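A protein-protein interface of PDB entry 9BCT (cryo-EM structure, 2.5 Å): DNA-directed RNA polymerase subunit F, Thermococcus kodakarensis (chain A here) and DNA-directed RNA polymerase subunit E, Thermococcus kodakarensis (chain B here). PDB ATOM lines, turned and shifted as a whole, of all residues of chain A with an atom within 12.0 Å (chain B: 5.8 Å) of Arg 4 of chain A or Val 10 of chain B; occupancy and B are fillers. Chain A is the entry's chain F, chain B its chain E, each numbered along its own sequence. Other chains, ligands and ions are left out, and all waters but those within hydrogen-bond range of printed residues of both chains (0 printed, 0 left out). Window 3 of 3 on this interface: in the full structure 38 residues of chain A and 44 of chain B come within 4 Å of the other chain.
The side-chain carboxylate (OD1) of Asp 9 of chain B lies within salt-bridge range of the guanidinium group (NE) of Arg 4 of chain A (3.8 Å). N of Gly 3 of chain A is in hydrogen-bond range of OH of Tyr 34 of chain B (3.3 Å). O of Lys 8 of chain B is in hydrogen-bond range of N of Arg 4 of chain A (3.1 Å). O of Lys 5 of chain A is in hydrogen-bond range of N of Lys 8 of chain B (3.3 Å).
The side-chain carboxylate of Asp 9 of chain B sits close to the side-chain hydroxyl of Tyr 34 of chain B (3.5 Å). The backbone carbonyl oxygen (O) of Ala 70 of chain B lies within hydrogen-bond range of the backbone NH (N) of Asp 9 of chain B, at 2.9 Å. The side-chain amino group (NZ) of Lys 8 of chain B is in salt-bridge range of the side-chain carboxylate (OE1) of Glu 69 of chain B (3.8 Å).
Among the printed residues, merely in contact across the chains: Ile 2 of chain A with Val 7 of chain B (3.3 Å), Ile 2 of chain A with Tyr 34 of chain B (3.5 Å), Gly 3 of chain A with Val 7 of chain B (3.7 Å), Gly 3 of chain A with Lys 8 of chain B (3.98 Å), Gly 3 of chain A with Asp 9 of chain B (3.4 Å), Arg 4 of chain A with Val 10 of chain B (3.5 Å) and Lys 5 of chain A with Val 7 of chain B (3.9 Å).
Of the printed residues of chain B, Gly 3 of chain A touches Val 7 (3.7 Å), Lys 8 (3.98 Å), Asp 9 (3.4 Å) and Tyr 34 (3.3 Å). Arg 4 of chain A touches just these residues of chain B: Lys 8, Asp 9 and Val 10. Of the printed residues of chain A, Val 7 of chain B touches Ile 2 (3.3 Å), Gly 3 (3.7 Å) and Lys 5 (3.9 Å). Of chain A, only Gly 3 and Arg 4 come within 4 Å of Asp 9 of chain B. Printed residues of chain A within 4 Å of Tyr 34 of chain B: Ile 2 and Gly 3. Tyr 67 of chain B touches none of the printed residues of chain A. No residue of chain A comes within 4 Å of Glu 69 of chain B. Ala 70 of chain B touches none of the printed residues of chain A. The nearest residue of chain B that does not touch Arg 4 of chain A is Val 7 of chain B (4.9 Å). The nearest residue of chain A that does not touch Val 10 of chain B is Gly 3 of chain A (6.1 Å).
Of the 8 printed residues of chain A, 4 touch a printed residue of chain B. Hydrophobic or aromatic side chains of chain A within 4 Å of the printed part of chain B: Ile 2. Of the 12 printed residues of chain B, 5 touch a printed residue of chain A. Along chain B the printed residues that touch a printed residue of chain A span positions 7 to 34. Among the printed residues, 11 pairs touch across the chains.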
ATOM      1  N   MET A   1      -4.093  36.403 -12.115  1.00  0.00           N
ATOM      2  CA  MET A   1      -3.902  35.285 -13.032  1.00  0.00           C
ATOM      3  C   MET A   1      -4.009  33.956 -12.293  1.00  0.00           C
ATOM      4  O   MET A   1      -3.212  33.665 -11.401  1.00  0.00           O
ATOM      5  CB  MET A   1      -2.545  35.393 -13.734  1.00  0.00           C
ATOM      6  CG  MET A   1      -2.089  34.130 -14.463  1.00  0.00           C
ATOM      7  SD  MET A   1      -2.653  34.002 -16.176  1.00  0.00           S
ATOM      8  CE  MET A   1      -4.277  33.269 -15.991  1.00  0.00           C
ATOM      9  N   ILE A   2      -5.001  33.155 -12.664  1.00  0.00           N
ATOM     10  CA  ILE A   2      -5.216  31.848 -12.055  1.00  0.00           C
ATOM     11  C   ILE A   2      -4.406  30.818 -12.832  1.00  0.00           C
ATOM     12  O   ILE A   2      -4.651  30.593 -14.022  1.00  0.00           O
ATOM     13  CB  ILE A   2      -6.706  31.478 -12.037  1.00  0.00           C
ATOM     14  CG1 ILE A   2      -7.475  32.404 -11.094  1.00  0.00           C
ATOM     15  CG2 ILE A   2      -6.889  30.026 -11.621  1.00  0.00           C
ATOM     16  CD1 ILE A   2      -7.236  32.119  -9.634  1.00  0.00           C
ATOM     17  N   GLY A   3      -3.439  30.201 -12.163  1.00  0.00           N
ATOM     18  CA  GLY A   3      -2.646  29.155 -12.775  1.00  0.00           C
ATOM     19  C   GLY A   3      -1.606  29.686 -13.739  1.00  0.00           C
ATOM     20  O   GLY A   3      -1.425  30.889 -13.929  1.00  0.00           O
ATOM     21  N   ARG A   4      -0.897  28.742 -14.363  1.00  0.00           N
ATOM     22  CA  ARG A   4       0.123  29.107 -15.340  1.00  0.00           C
ATOM     23  C   ARG A   4      -0.505  29.645 -16.621  1.00  0.00           C
ATOM     24  O   ARG A   4      -0.033  30.642 -17.179  1.00  0.00           O
ATOM     25  CB  ARG A   4       1.013  27.904 -15.643  1.00  0.00           C
ATOM     26  CG  ARG A   4       1.698  27.317 -14.420  1.00  0.00           C
ATOM     27  CD  ARG A   4       2.631  28.327 -13.773  1.00  0.00           C
ATOM     28  NE  ARG A   4       3.296  27.785 -12.596  1.00  0.00           N
ATOM     29  CZ  ARG A   4       4.391  27.039 -12.630  1.00  0.00           C
ATOM     30  NH1 ARG A   4       4.978  26.725 -13.774  1.00  0.00           N
ATOM     31  NH2 ARG A   4       4.913  26.599 -11.489  1.00  0.00           N
ATOM     32  N   LYS A   5      -1.566  29.001 -17.100  1.00  0.00           N
ATOM     33  CA  LYS A   5      -2.234  29.430 -18.318  1.00  0.00           C
ATOM     34  C   LYS A   5      -3.692  28.995 -18.270  1.00  0.00           C
ATOM     35  O   LYS A   5      -4.067  28.094 -17.516  1.00  0.00           O
ATOM     36  CB  LYS A   5      -1.540  28.871 -19.568  1.00  0.00           C
ATOM     37  CG  LYS A   5      -2.071  27.528 -20.039  1.00  0.00           C
ATOM     38  CD  LYS A   5      -1.928  27.377 -21.544  1.00  0.00           C
ATOM     39  CE  LYS A   5      -0.611  26.713 -21.909  1.00  0.00           C
ATOM     40  NZ  LYS A   5      -0.529  25.321 -21.387  1.00  0.00           N
ATOM     41  N   LYS A   6      -4.510  29.654 -19.086  1.00  0.00           N
ATOM     42  CA  LYS A   6      -5.934  29.370 -19.181  1.00  0.00           C
ATOM     43  C   LYS A   6      -6.212  28.616 -20.474  1.00  0.00           C
ATOM     44  O   LYS A   6      -5.818  29.066 -21.556  1.00  0.00           O
ATOM     45  CB  LYS A   6      -6.755  30.661 -19.134  1.00  0.00           C
ATOM     46  CG  LYS A   6      -8.215  30.458 -18.770  1.00  0.00           C
ATOM     47  CD  LYS A   6      -8.838  31.743 -18.248  1.00  0.00           C
ATOM     48  CE  LYS A   6      -8.685  32.878 -19.247  1.00  0.00           C
ATOM     49  NZ  LYS A   6      -9.722  33.929 -19.056  1.00  0.00           N
ATOM     50  N   LEU A   7      -6.887  27.473 -20.359  1.00  0.00           N
ATOM     51  CA  LEU A   7      -7.192  26.647 -21.523  1.00  0.00           C
ATOM     52  C   LEU A   7      -8.522  27.042 -22.159  1.00  0.00           C
ATOM     53  O   LEU A   7      -8.569  27.419 -23.334  1.00  0.00           O
ATOM     54  CB  LEU A   7      -7.204  25.167 -21.125  1.00  0.00           C
ATOM     55  CG  LEU A   7      -5.877  24.576 -20.647  1.00  0.00           C
ATOM     56  CD1 LEU A   7      -5.983  23.067 -20.508  1.00  0.00           C
ATOM     57  CD2 LEU A   7      -4.749  24.949 -21.596  1.00  0.00           C
ATOM     58  N   GLU A   8      -9.608  26.962 -21.393  1.00  0.00           N
ATOM     59  CA  GLU A   8     -10.939  27.294 -21.881  1.00  0.00           C
ATOM     60  C   GLU A   8     -11.586  28.304 -20.947  1.00  0.00           C
ATOM     61  O   GLU A   8     -11.472  28.192 -19.723  1.00  0.00           O
ATOM     62  CB  GLU A   8     -11.822  26.045 -21.991  1.00  0.00           C
ATOM     63  CG  GLU A   8     -11.235  24.939 -22.853  1.00  0.00           C
ATOM     64  CD  GLU A   8     -12.166  23.752 -22.990  1.00  0.00           C
ATOM     65  OE1 GLU A   8     -13.181  23.702 -22.262  1.00  0.00           O
ATOM     66  OE2 GLU A   8     -11.885  22.867 -23.826  1.00  0.00           O
ATOM     67  N   VAL B   7      -8.217  25.618 -16.101  1.00  0.00           N
ATOM     68  CA  VAL B   7      -6.923  26.191 -15.756  1.00  0.00           C
ATOM     69  C   VAL B   7      -5.933  25.063 -15.510  1.00  0.00           C
ATOM     70  O   VAL B   7      -6.223  24.129 -14.754  1.00  0.00           O
ATOM     71  CB  VAL B   7      -7.028  27.107 -14.522  1.00  0.00           C
ATOM     72  CG1 VAL B   7      -5.649  27.475 -14.012  1.00  0.00           C
ATOM     73  CG2 VAL B   7      -7.829  28.355 -14.856  1.00  0.00           C
ATOM     74  N   LYS B   8      -4.774  25.151 -16.156  1.00  0.00           N
ATOM     75  CA  LYS B   8      -3.666  24.233 -15.929  1.00  0.00           C
ATOM     76  C   LYS B   8      -2.647  24.912 -15.023  1.00  0.00           C
ATOM     77  O   LYS B   8      -2.274  26.067 -15.258  1.00  0.00           O
ATOM     78  CB  LYS B   8      -3.030  23.818 -17.257  1.00  0.00           C
ATOM     79  CG  LYS B   8      -1.519  23.665 -17.227  1.00  0.00           C
ATOM     80  CD  LYS B   8      -0.989  23.183 -18.566  1.00  0.00           C
ATOM     81  CE  LYS B   8      -1.639  21.872 -18.980  1.00  0.00           C
ATOM     82  NZ  LYS B   8      -0.753  21.067 -19.864  1.00  0.00           N
ATOM     83  N   ASP B   9      -2.211  24.205 -13.982  1.00  0.00           N
ATOM     84  CA  ASP B   9      -1.340  24.804 -12.981  1.00  0.00           C
ATOM     85  C   ASP B   9      -0.515  23.722 -12.300  1.00  0.00           C
ATOM     86  O   ASP B   9      -0.857  22.536 -12.325  1.00  0.00           O
ATOM     87  CB  ASP B   9      -2.152  25.591 -11.942  1.00  0.00           C
ATOM     88  CG  ASP B   9      -1.287  26.486 -11.075  1.00  0.00           C
ATOM     89  OD1 ASP B   9      -0.128  26.750 -11.459  1.00  0.00           O
ATOM     90  OD2 ASP B   9      -1.767  26.926 -10.010  1.00  0.00           O
ATOM     91  N   VAL B  10       0.579  24.153 -11.680  1.00  0.00           N
ATOM     92  CA  VAL B  10       1.417  23.280 -10.869  1.00  0.00           C
ATOM     93  C   VAL B  10       0.909  23.336  -9.434  1.00  0.00           C
ATOM     94  O   VAL B  10       0.858  24.409  -8.822  1.00  0.00           O
ATOM     95  CB  VAL B  10       2.894  23.692 -10.951  1.00  0.00           C
ATOM     96  CG1 VAL B  10       3.734  22.835 -10.019  1.00  0.00           C
ATOM     97  CG2 VAL B  10       3.396  23.582 -12.382  1.00  0.00           C
ATOM     98  N   VAL B  11       0.533  22.179  -8.898  1.00  0.00           N
ATOM     99  CA  VAL B  11      -0.038  22.054  -7.563  1.00  0.00           C
ATOM    100  C   VAL B  11       0.977  21.348  -6.677  1.00  0.00           C
ATOM    101  O   VAL B  11       1.535  20.313  -7.063  1.00  0.00           O
ATOM    102  CB  VAL B  11      -1.371  21.285  -7.594  1.00  0.00           C
ATOM    103  CG1 VAL B  11      -2.054  21.352  -6.240  1.00  0.00           C
ATOM    104  CG2 VAL B  11      -2.276  21.839  -8.683  1.00  0.00           C
ATOM    105  N   ARG B  12       1.219  21.909  -5.496  1.00  0.00           N
ATOM    106  CA  ARG B  12       2.179  21.367  -4.546  1.00  0.00           C
ATOM    107  C   ARG B  12       1.437  20.549  -3.496  1.00  0.00           C
ATOM    108  O   ARG B  12       0.594  21.085  -2.769  1.00  0.00           O
ATOM    109  CB  ARG B  12       2.980  22.491  -3.889  1.00  0.00           C
ATOM    110  CG  ARG B  12       3.861  22.038  -2.743  1.00  0.00           C
ATOM    111  CD  ARG B  12       4.297  23.209  -1.880  1.00  0.00           C
ATOM    112  NE  ARG B  12       5.087  22.777  -0.734  1.00  0.00           N
ATOM    113  CZ  ARG B  12       4.575  22.352   0.412  1.00  0.00           C
ATOM    114  NH1 ARG B  12       3.268  22.288   0.604  1.00  0.00           N
ATOM    115  NH2 ARG B  12       5.395  21.978   1.390  1.00  0.00           N
ATOM    116  N   LEU B  30      -5.622  23.235  -4.037  1.00  0.00           N
ATOM    117  CA  LEU B  30      -6.131  24.343  -4.840  1.00  0.00           C
ATOM    118  C   LEU B  30      -7.262  25.075  -4.126  1.00  0.00           C
ATOM    119  O   LEU B  30      -7.377  26.300  -4.233  1.00  0.00           O
ATOM    120  CB  LEU B  30      -6.594  23.835  -6.205  1.00  0.00           C
ATOM    121  CG  LEU B  30      -5.477  23.374  -7.142  1.00  0.00           C
ATOM    122  CD1 LEU B  30      -6.014  22.396  -8.173  1.00  0.00           C
ATOM    123  CD2 LEU B  30      -4.804  24.561  -7.811  1.00  0.00           C
ATOM    124  N   TYR B  34      -6.387  28.978  -3.734  1.00  0.00           N
ATOM    125  CA  TYR B  34      -6.931  29.964  -4.657  1.00  0.00           C
ATOM    126  C   TYR B  34      -8.321  30.463  -4.288  1.00  0.00           C
ATOM    127  O   TYR B  34      -8.702  31.556  -4.721  1.00  0.00           O
ATOM    128  CB  TYR B  34      -6.973  29.389  -6.077  1.00  0.00           C
ATOM    129  CG  TYR B  34      -5.703  29.608  -6.866  1.00  0.00           C
ATOM    130  CD1 TYR B  34      -5.176  30.882  -7.029  1.00  0.00           C
ATOM    131  CD2 TYR B  34      -5.034  28.543  -7.454  1.00  0.00           C
ATOM    132  CE1 TYR B  34      -4.020  31.090  -7.753  1.00  0.00           C
ATOM    133  CE2 TYR B  34      -3.876  28.740  -8.180  1.00  0.00           C
ATOM    134  CZ  TYR B  34      -3.374  30.015  -8.325  1.00  0.00           C
ATOM    135  OH  TYR B  34      -2.221  30.217  -9.046  1.00  0.00           O
ATOM    136  N   TYR B  67       5.282  18.189  -6.804  1.00  0.00           N
ATOM    137  CA  TYR B  67       4.625  19.143  -7.689  1.00  0.00           C
ATOM    138  C   TYR B  67       4.020  18.402  -8.875  1.00  0.00           C
ATOM    139  O   TYR B  67       4.726  17.684  -9.589  1.00  0.00           O
ATOM    140  CB  TYR B  67       5.612  20.211  -8.161  1.00  0.00           C
ATOM    141  CG  TYR B  67       6.073  21.138  -7.059  1.00  0.00           C
ATOM    142  CD1 TYR B  67       7.116  20.781  -6.214  1.00  0.00           C
ATOM    143  CD2 TYR B  67       5.462  22.370  -6.860  1.00  0.00           C
ATOM    144  CE1 TYR B  67       7.538  21.624  -5.205  1.00  0.00           C
ATOM    145  CE2 TYR B  67       5.879  23.219  -5.855  1.00  0.00           C
ATOM    146  CZ  TYR B  67       6.917  22.842  -5.030  1.00  0.00           C
ATOM    147  OH  TYR B  67       7.336  23.684  -4.026  1.00  0.00           O
ATOM    148  N   HIS B  68       2.718  18.587  -9.085  1.00  0.00           N
ATOM    149  CA  HIS B  68       1.978  17.911 -10.140  1.00  0.00           C
ATOM    150  C   HIS B  68       1.383  18.932 -11.098  1.00  0.00           C
ATOM    151  O   HIS B  68       0.852  19.960 -10.670  1.00  0.00           O
ATOM    152  CB  HIS B  68       0.856  17.043  -9.561  1.00  0.00           C
ATOM    153  CG  HIS B  68       1.333  15.770  -8.936  1.00  0.00           C
ATOM    154  ND1 HIS B  68       1.104  14.533  -9.501  1.00  0.00           N
ATOM    155  CD2 HIS B  68       2.017  15.540  -7.791  1.00  0.00           C
ATOM    156  CE1 HIS B  68       1.631  13.596  -8.733  1.00  0.00           C
ATOM    157  NE2 HIS B  68       2.191  14.181  -7.689  1.00  0.00           N
ATOM    158  N   GLU B  69       1.458  18.643 -12.393  1.00  0.00           N
ATOM    159  CA  GLU B  69       0.860  19.496 -13.415  1.00  0.00           C
ATOM    160  C   GLU B  69      -0.580  19.044 -13.631  1.00  0.00           C
ATOM    161  O   GLU B  69      -0.823  18.002 -14.248  1.00  0.00           O
ATOM    162  CB  GLU B  69       1.667  19.425 -14.709  1.00  0.00           C
ATOM    163  CG  GLU B  69       2.206  20.765 -15.184  1.00  0.00           C
ATOM    164  CD  GLU B  69       1.192  21.551 -15.988  1.00  0.00           C
ATOM    165  OE1 GLU B  69       0.040  21.085 -16.115  1.00  0.00           O
ATOM    166  OE2 GLU B  69       1.547  22.637 -16.493  1.00  0.00           O
ATOM    167  N   ALA B  70      -1.536  19.821 -13.126  1.00  0.00           N
ATOM    168  CA  ALA B  70      -2.935  19.417 -13.095  1.00  0.00           C
ATOM    169  C   ALA B  70      -3.814  20.451 -13.783  1.00  0.00           C
ATOM    170  O   ALA B  70      -3.575  21.658 -13.677  1.00  0.00           O
ATOM    171  CB  ALA B  70      -3.413  19.210 -11.655  1.00  0.00           C
